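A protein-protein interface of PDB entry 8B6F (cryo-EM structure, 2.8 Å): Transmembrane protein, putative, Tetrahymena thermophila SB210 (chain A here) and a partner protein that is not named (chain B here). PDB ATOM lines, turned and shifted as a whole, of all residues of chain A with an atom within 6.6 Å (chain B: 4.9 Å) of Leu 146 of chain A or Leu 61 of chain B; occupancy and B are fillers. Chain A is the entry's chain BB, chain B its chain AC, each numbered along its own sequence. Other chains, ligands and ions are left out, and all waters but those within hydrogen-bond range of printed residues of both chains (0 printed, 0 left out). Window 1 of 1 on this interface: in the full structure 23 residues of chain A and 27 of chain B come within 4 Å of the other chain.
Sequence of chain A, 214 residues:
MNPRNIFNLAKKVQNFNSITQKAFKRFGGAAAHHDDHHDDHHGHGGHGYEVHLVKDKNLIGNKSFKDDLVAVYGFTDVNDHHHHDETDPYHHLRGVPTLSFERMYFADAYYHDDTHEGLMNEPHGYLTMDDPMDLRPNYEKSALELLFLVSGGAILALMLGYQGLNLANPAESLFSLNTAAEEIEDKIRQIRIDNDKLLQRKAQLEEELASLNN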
ATOM      1  N   LYS A 141       1.800 -17.083 -37.583  1.00  0.00           N
ATOM      2  CA  LYS A 141       3.008 -17.818 -37.944  1.00  0.00           C
ATOM      3  C   LYS A 141       4.031 -17.785 -36.818  1.00  0.00           C
ATOM      4  O   LYS A 141       4.653 -18.805 -36.503  1.00  0.00           O
ATOM      5  CB  LYS A 141       3.608 -17.249 -39.228  1.00  0.00           C
ATOM      6  CG  LYS A 141       4.973 -17.827 -39.585  1.00  0.00           C
ATOM      7  CD  LYS A 141       5.465 -17.295 -40.920  1.00  0.00           C
ATOM      8  CE  LYS A 141       6.861 -17.806 -41.238  1.00  0.00           C
ATOM      9  NZ  LYS A 141       7.324 -17.354 -42.579  1.00  0.00           N
ATOM     10  N   SER A 142       4.221 -16.619 -36.202  1.00  0.00           N
ATOM     11  CA  SER A 142       5.158 -16.514 -35.090  1.00  0.00           C
ATOM     12  C   SER A 142       4.713 -17.374 -33.916  1.00  0.00           C
ATOM     13  O   SER A 142       5.542 -17.999 -33.245  1.00  0.00           O
ATOM     14  CB  SER A 142       5.308 -15.054 -34.664  1.00  0.00           C
ATOM     15  OG  SER A 142       4.080 -14.531 -34.194  1.00  0.00           O
ATOM     16  N   ALA A 143       3.409 -17.408 -33.640  1.00  0.00           N
ATOM     17  CA  ALA A 143       2.916 -18.230 -32.543  1.00  0.00           C
ATOM     18  C   ALA A 143       3.193 -19.708 -32.785  1.00  0.00           C
ATOM     19  O   ALA A 143       3.634 -20.420 -31.876  1.00  0.00           O
ATOM     20  CB  ALA A 143       1.419 -17.995 -32.352  1.00  0.00           C
ATOM     21  N   LEU A 144       2.938 -20.192 -34.001  1.00  0.00           N
ATOM     22  CA  LEU A 144       3.172 -21.603 -34.285  1.00  0.00           C
ATOM     23  C   LEU A 144       4.658 -21.931 -34.278  1.00  0.00           C
ATOM     24  O   LEU A 144       5.061 -23.000 -33.807  1.00  0.00           O
ATOM     25  CB  LEU A 144       2.539 -21.983 -35.619  1.00  0.00           C
ATOM     26  CG  LEU A 144       1.009 -21.935 -35.658  1.00  0.00           C
ATOM     27  CD1 LEU A 144       0.528 -22.432 -36.986  1.00  0.00           C
ATOM     28  CD2 LEU A 144       0.387 -22.757 -34.542  1.00  0.00           C
ATOM     29  N   GLU A 145       5.490 -21.030 -34.804  1.00  0.00           N
ATOM     30  CA  GLU A 145       6.931 -21.243 -34.744  1.00  0.00           C
ATOM     31  C   GLU A 145       7.410 -21.288 -33.302  1.00  0.00           C
ATOM     32  O   GLU A 145       8.269 -22.102 -32.946  1.00  0.00           O
ATOM     33  CB  GLU A 145       7.659 -20.145 -35.517  1.00  0.00           C
ATOM     34  CG  GLU A 145       7.477 -20.228 -37.019  1.00  0.00           C
ATOM     35  CD  GLU A 145       8.151 -19.084 -37.745  1.00  0.00           C
ATOM     36  OE1 GLU A 145       8.559 -18.114 -37.073  1.00  0.00           O
ATOM     37  OE2 GLU A 145       8.276 -19.155 -38.987  1.00  0.00           O
ATOM     38  N   LEU A 146       6.869 -20.411 -32.457  1.00  0.00           N
ATOM     39  CA  LEU A 146       7.226 -20.434 -31.045  1.00  0.00           C
ATOM     40  C   LEU A 146       6.801 -21.744 -30.397  1.00  0.00           C
ATOM     41  O   LEU A 146       7.545 -22.318 -29.594  1.00  0.00           O
ATOM     42  CB  LEU A 146       6.587 -19.246 -30.328  1.00  0.00           C
ATOM     43  CG  LEU A 146       6.857 -19.129 -28.829  1.00  0.00           C
ATOM     44  CD1 LEU A 146       8.342 -18.953 -28.559  1.00  0.00           C
ATOM     45  CD2 LEU A 146       6.064 -17.975 -28.248  1.00  0.00           C
ATOM     46  N   LEU A 147       5.608 -22.237 -30.736  1.00  0.00           N
ATOM     47  CA  LEU A 147       5.162 -23.514 -30.193  1.00  0.00           C
ATOM     48  C   LEU A 147       6.111 -24.636 -30.592  1.00  0.00           C
ATOM     49  O   LEU A 147       6.505 -25.460 -29.759  1.00  0.00           O
ATOM     50  CB  LEU A 147       3.739 -23.811 -30.668  1.00  0.00           C
ATOM     51  CG  LEU A 147       3.161 -25.174 -30.284  1.00  0.00           C
ATOM     52  CD1 LEU A 147       3.165 -25.362 -28.778  1.00  0.00           C
ATOM     53  CD2 LEU A 147       1.757 -25.328 -30.835  1.00  0.00           C
ATOM     54  N   PHE A 148       6.475 -24.698 -31.874  1.00  0.00           N
ATOM     55  CA  PHE A 148       7.411 -25.720 -32.330  1.00  0.00           C
ATOM     56  C   PHE A 148       8.742 -25.614 -31.598  1.00  0.00           C
ATOM     57  O   PHE A 148       9.274 -26.611 -31.096  1.00  0.00           O
ATOM     58  CB  PHE A 148       7.629 -25.597 -33.839  1.00  0.00           C
ATOM     59  CG  PHE A 148       6.894 -26.624 -34.646  1.00  0.00           C
ATOM     60  CD1 PHE A 148       7.316 -27.941 -34.662  1.00  0.00           C
ATOM     61  CD2 PHE A 148       5.797 -26.266 -35.411  1.00  0.00           C
ATOM     62  CE1 PHE A 148       6.648 -28.889 -35.410  1.00  0.00           C
ATOM     63  CE2 PHE A 148       5.125 -27.208 -36.163  1.00  0.00           C
ATOM     64  CZ  PHE A 148       5.550 -28.521 -36.161  1.00  0.00           C
ATOM     65  N   LEU A 149       9.298 -24.402 -31.532  1.00  0.00           N
ATOM     66  CA  LEU A 149      10.612 -24.219 -30.923  1.00  0.00           C
ATOM     67  C   LEU A 149      10.601 -24.574 -29.443  1.00  0.00           C
ATOM     68  O   LEU A 149      11.541 -25.201 -28.943  1.00  0.00           O
ATOM     69  CB  LEU A 149      11.079 -22.778 -31.117  1.00  0.00           C
ATOM     70  CG  LEU A 149      11.417 -22.344 -32.543  1.00  0.00           C
ATOM     71  CD1 LEU A 149      11.673 -20.848 -32.578  1.00  0.00           C
ATOM     72  CD2 LEU A 149      12.621 -23.109 -33.068  1.00  0.00           C
ATOM     73  N   VAL A 150       9.551 -24.180 -28.724  1.00  0.00           N
ATOM     74  CA  VAL A 150       9.498 -24.460 -27.293  1.00  0.00           C
ATOM     75  C   VAL A 150       9.315 -25.952 -27.049  1.00  0.00           C
ATOM     76  O   VAL A 150       9.893 -26.515 -26.113  1.00  0.00           O
ATOM     77  CB  VAL A 150       8.396 -23.627 -26.619  1.00  0.00           C
ATOM     78  CG1 VAL A 150       8.197 -24.075 -25.183  1.00  0.00           C
ATOM     79  CG2 VAL A 150       8.745 -22.152 -26.666  1.00  0.00           C
ATOM     80  N   SER A 151       8.505 -26.616 -27.875  1.00  0.00           N
ATOM     81  CA  SER A 151       8.373 -28.062 -27.751  1.00  0.00           C
ATOM     82  C   SER A 151       9.714 -28.745 -27.978  1.00  0.00           C
ATOM     83  O   SER A 151      10.111 -29.632 -27.215  1.00  0.00           O
ATOM     84  CB  SER A 151       7.339 -28.581 -28.748  1.00  0.00           C
ATOM     85  OG  SER A 151       7.322 -29.996 -28.752  1.00  0.00           O
ATOM     86  N   ILE B  57      -4.761 -16.117 -26.831  1.00  0.00           N
ATOM     87  CA  ILE B  57      -3.849 -17.017 -27.533  1.00  0.00           C
ATOM     88  C   ILE B  57      -2.597 -17.263 -26.703  1.00  0.00           C
ATOM     89  O   ILE B  57      -2.197 -18.410 -26.479  1.00  0.00           O
ATOM     90  CB  ILE B  57      -3.501 -16.449 -28.921  1.00  0.00           C
ATOM     91  CG1 ILE B  57      -4.677 -16.604 -29.887  1.00  0.00           C
ATOM     92  CG2 ILE B  57      -2.248 -17.110 -29.497  1.00  0.00           C
ATOM     93  CD1 ILE B  57      -5.110 -18.039 -30.123  1.00  0.00           C
ATOM     94  N   PHE B  58      -1.964 -16.196 -26.236  1.00  0.00           N
ATOM     95  CA  PHE B  58      -0.687 -16.305 -25.550  1.00  0.00           C
ATOM     96  C   PHE B  58      -0.839 -16.384 -24.042  1.00  0.00           C
ATOM     97  O   PHE B  58       0.149 -16.238 -23.320  1.00  0.00           O
ATOM     98  CB  PHE B  58       0.225 -15.150 -25.956  1.00  0.00           C
ATOM     99  CG  PHE B  58       0.549 -15.150 -27.420  1.00  0.00           C
ATOM    100  CD1 PHE B  58       1.322 -16.157 -27.973  1.00  0.00           C
ATOM    101  CD2 PHE B  58       0.059 -14.164 -28.245  1.00  0.00           C
ATOM    102  CE1 PHE B  58       1.607 -16.168 -29.328  1.00  0.00           C
ATOM    103  CE2 PHE B  58       0.338 -14.166 -29.598  1.00  0.00           C
ATOM    104  CZ  PHE B  58       1.115 -15.167 -30.140  1.00  0.00           C
ATOM    105  N   GLY B  59      -2.054 -16.600 -23.555  1.00  0.00           N
ATOM    106  CA  GLY B  59      -2.237 -17.151 -22.233  1.00  0.00           C
ATOM    107  C   GLY B  59      -2.321 -18.656 -22.334  1.00  0.00           C
ATOM    108  O   GLY B  59      -1.738 -19.383 -21.526  1.00  0.00           O
ATOM    109  N   ILE B  60      -3.067 -19.136 -23.329  1.00  0.00           N
ATOM    110  CA  ILE B  60      -3.166 -20.573 -23.563  1.00  0.00           C
ATOM    111  C   ILE B  60      -1.793 -21.160 -23.868  1.00  0.00           C
ATOM    112  O   ILE B  60      -1.414 -22.210 -23.339  1.00  0.00           O
ATOM    113  CB  ILE B  60      -4.163 -20.855 -24.703  1.00  0.00           C
ATOM    114  CG1 ILE B  60      -5.587 -20.490 -24.273  1.00  0.00           C
ATOM    115  CG2 ILE B  60      -4.093 -22.317 -25.142  1.00  0.00           C
ATOM    116  CD1 ILE B  60      -6.602 -20.513 -25.405  1.00  0.00           C
ATOM    117  N   LEU B  61      -1.032 -20.496 -24.743  1.00  0.00           N
ATOM    118  CA  LEU B  61       0.282 -21.004 -25.126  1.00  0.00           C
ATOM    119  C   LEU B  61       1.268 -21.026 -23.960  1.00  0.00           C
ATOM    120  O   LEU B  61       1.956 -22.029 -23.738  1.00  0.00           O
ATOM    121  CB  LEU B  61       0.840 -20.159 -26.273  1.00  0.00           C
ATOM    122  CG  LEU B  61       2.094 -20.692 -26.973  1.00  0.00           C
ATOM    123  CD1 LEU B  61       1.835 -22.034 -27.640  1.00  0.00           C
ATOM    124  CD2 LEU B  61       2.613 -19.681 -27.982  1.00  0.00           C
ATOM    125  N   ILE B  62       1.352 -19.934 -23.200  1.00  0.00           N
ATOM    126  CA  ILE B  62       2.266 -19.899 -22.058  1.00  0.00           C
ATOM    127  C   ILE B  62       1.834 -20.867 -20.965  1.00  0.00           C
ATOM    128  O   ILE B  62       2.669 -21.536 -20.347  1.00  0.00           O
ATOM    129  CB  ILE B  62       2.400 -18.465 -21.514  1.00  0.00           C
ATOM    130  CG1 ILE B  62       2.859 -17.515 -22.622  1.00  0.00           C
ATOM    131  CG2 ILE B  62       3.377 -18.432 -20.341  1.00  0.00           C
ATOM    132  CD1 ILE B  62       2.866 -16.058 -22.214  1.00  0.00           C
ATOM    133  N   SER B  63       0.532 -20.963 -20.705  1.00  0.00           N
ATOM    134  CA  SER B  63       0.046 -21.984 -19.786  1.00  0.00           C
ATOM    135  C   SER B  63       0.328 -23.391 -20.288  1.00  0.00           C
ATOM    136  O   SER B  63       0.555 -24.300 -19.483  1.00  0.00           O
ATOM    137  CB  SER B  63      -1.446 -21.785 -19.553  1.00  0.00           C
ATOM    138  OG  SER B  63      -1.662 -20.519 -18.961  1.00  0.00           O
ATOM    139  N   PHE B  64       0.330 -23.593 -21.604  1.00  0.00           N
ATOM    140  CA  PHE B  64       0.692 -24.901 -22.133  1.00  0.00           C
ATOM    141  C   PHE B  64       2.157 -25.216 -21.869  1.00  0.00           C
ATOM    142  O   PHE B  64       2.496 -26.346 -21.499  1.00  0.00           O
ATOM    143  CB  PHE B  64       0.386 -24.963 -23.628  1.00  0.00           C
ATOM    144  CG  PHE B  64       0.870 -26.216 -24.292  1.00  0.00           C
ATOM    145  CD1 PHE B  64       0.353 -27.450 -23.935  1.00  0.00           C
ATOM    146  CD2 PHE B  64       1.829 -26.157 -25.289  1.00  0.00           C
ATOM    147  CE1 PHE B  64       0.793 -28.603 -24.550  1.00  0.00           C
ATOM    148  CE2 PHE B  64       2.275 -27.306 -25.908  1.00  0.00           C
ATOM    149  CZ  PHE B  64       1.756 -28.531 -25.539  1.00  0.00           C
ATOM    150  N   PHE B  65       3.041 -24.232 -22.038  1.00  0.00           N
ATOM    151  CA  PHE B  65       4.447 -24.444 -21.714  1.00  0.00           C
ATOM    152  C   PHE B  65       4.624 -24.767 -20.236  1.00  0.00           C
ATOM    153  O   PHE B  65       5.343 -25.703 -19.873  1.00  0.00           O
ATOM    154  CB  PHE B  65       5.260 -23.206 -22.092  1.00  0.00           C
ATOM    155  CG  PHE B  65       5.218 -22.876 -23.556  1.00  0.00           C
ATOM    156  CD1 PHE B  65       4.965 -23.856 -24.504  1.00  0.00           C
ATOM    157  CD2 PHE B  65       5.448 -21.581 -23.987  1.00  0.00           C
ATOM    158  CE1 PHE B  65       4.931 -23.547 -25.849  1.00  0.00           C
ATOM    159  CE2 PHE B  65       5.417 -21.267 -25.331  1.00  0.00           C
ATOM    160  CZ  PHE B  65       5.160 -22.250 -26.263  1.00  0.00           C
ATOM    161  N   PHE B 131      -5.891 -24.704 -28.347  1.00  0.00           N
ATOM    162  CA  PHE B 131      -5.062 -23.808 -29.146  1.00  0.00           C
ATOM    163  C   PHE B 131      -5.413 -23.920 -30.626  1.00  0.00           C
ATOM    164  O   PHE B 131      -5.532 -22.909 -31.327  1.00  0.00           O
ATOM    165  CB  PHE B 131      -3.585 -24.124 -28.906  1.00  0.00           C
ATOM    166  CG  PHE B 131      -2.640 -23.162 -29.564  1.00  0.00           C
ATOM    167  CD1 PHE B 131      -2.443 -21.897 -29.037  1.00  0.00           C
ATOM    168  CD2 PHE B 131      -1.932 -23.529 -30.695  1.00  0.00           C
ATOM    169  CE1 PHE B 131      -1.568 -21.011 -29.633  1.00  0.00           C
ATOM    170  CE2 PHE B 131      -1.056 -22.647 -31.296  1.00  0.00           C
ATOM    171  CZ  PHE B 131      -0.873 -21.387 -30.764  1.00  0.00           C
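Phe 58 of chain B touches Ala 143 of chain A.
CE2 of Phe 131 of chain B touches CD2 of Leu 144 of chain A, 3.6 Å away.
Leu 146 of chain A touches Leu 61 of chain B.
Leu 61 of chain B touches Leu 147 of chain A (CD1 to CD1, 3.8 Å).
CE2 of Phe 64 of chain B touches CD1 of Leu 147 of chain A, at 3.6 Å.
CE1 of Phe 65 of chain B touches CD1 of Leu 147 of chain A (3.9 Å).
Phe 131 of chain B touches Leu 147 of chain A (CE2 to CD2, 3.9 Å).
Val 150 of chain A touches Phe 65 of chain B.
Printed residues of chain B within 4 Å of Ala 143 of chain A: Phe 58.
Leu 146 of chain A touches just one residue of chain B: Leu 61 (3.9 Å).
Phe 148 of chain A touches none of the printed residues of chain B.
Leu 149 of chain A touches none of the printed residues of chain B.
Printed residues of chain A within 4 Å of Phe 58 of chain B: Ala 143 (3.5 Å).
Of chain A, only Leu 146 (3.9 Å) and Leu 147 (3.8 Å) come within 4 Å of Leu 61 of chain B.
Printed residues of chain A within 4 Å of Phe 64 of chain B: Leu 147 (3.6 Å).
Of the printed residues of chain A, Phe 65 of chain B touches Leu 147 (3.9 Å) and Val 150 (3.3 Å).
The nearest residue of chain B that does not touch Leu 146 of chain A is Phe 65 of chain B (4.1 Å).
The nearest residue of chain A that does not touch Leu 61 of chain B is Ala 143 of chain A (4.1 Å).
The nearest printed residue of chain A that does not touch Phe 58 of chain B is Leu 146 of chain A (4.9 Å).
Hydrophobic or aromatic side chains of chain A that line the printed part of chain B: Ala 143, Leu 144, Leu 146, Leu 147 and Val 150.
Along chain A the printed residues that touch a printed residue of chain B span positions 143 to 150.
Among the printed residues, no Asp or Glu carboxylate lies within 4 Å of a Lys or Arg side-chain nitrogen of the other chain.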
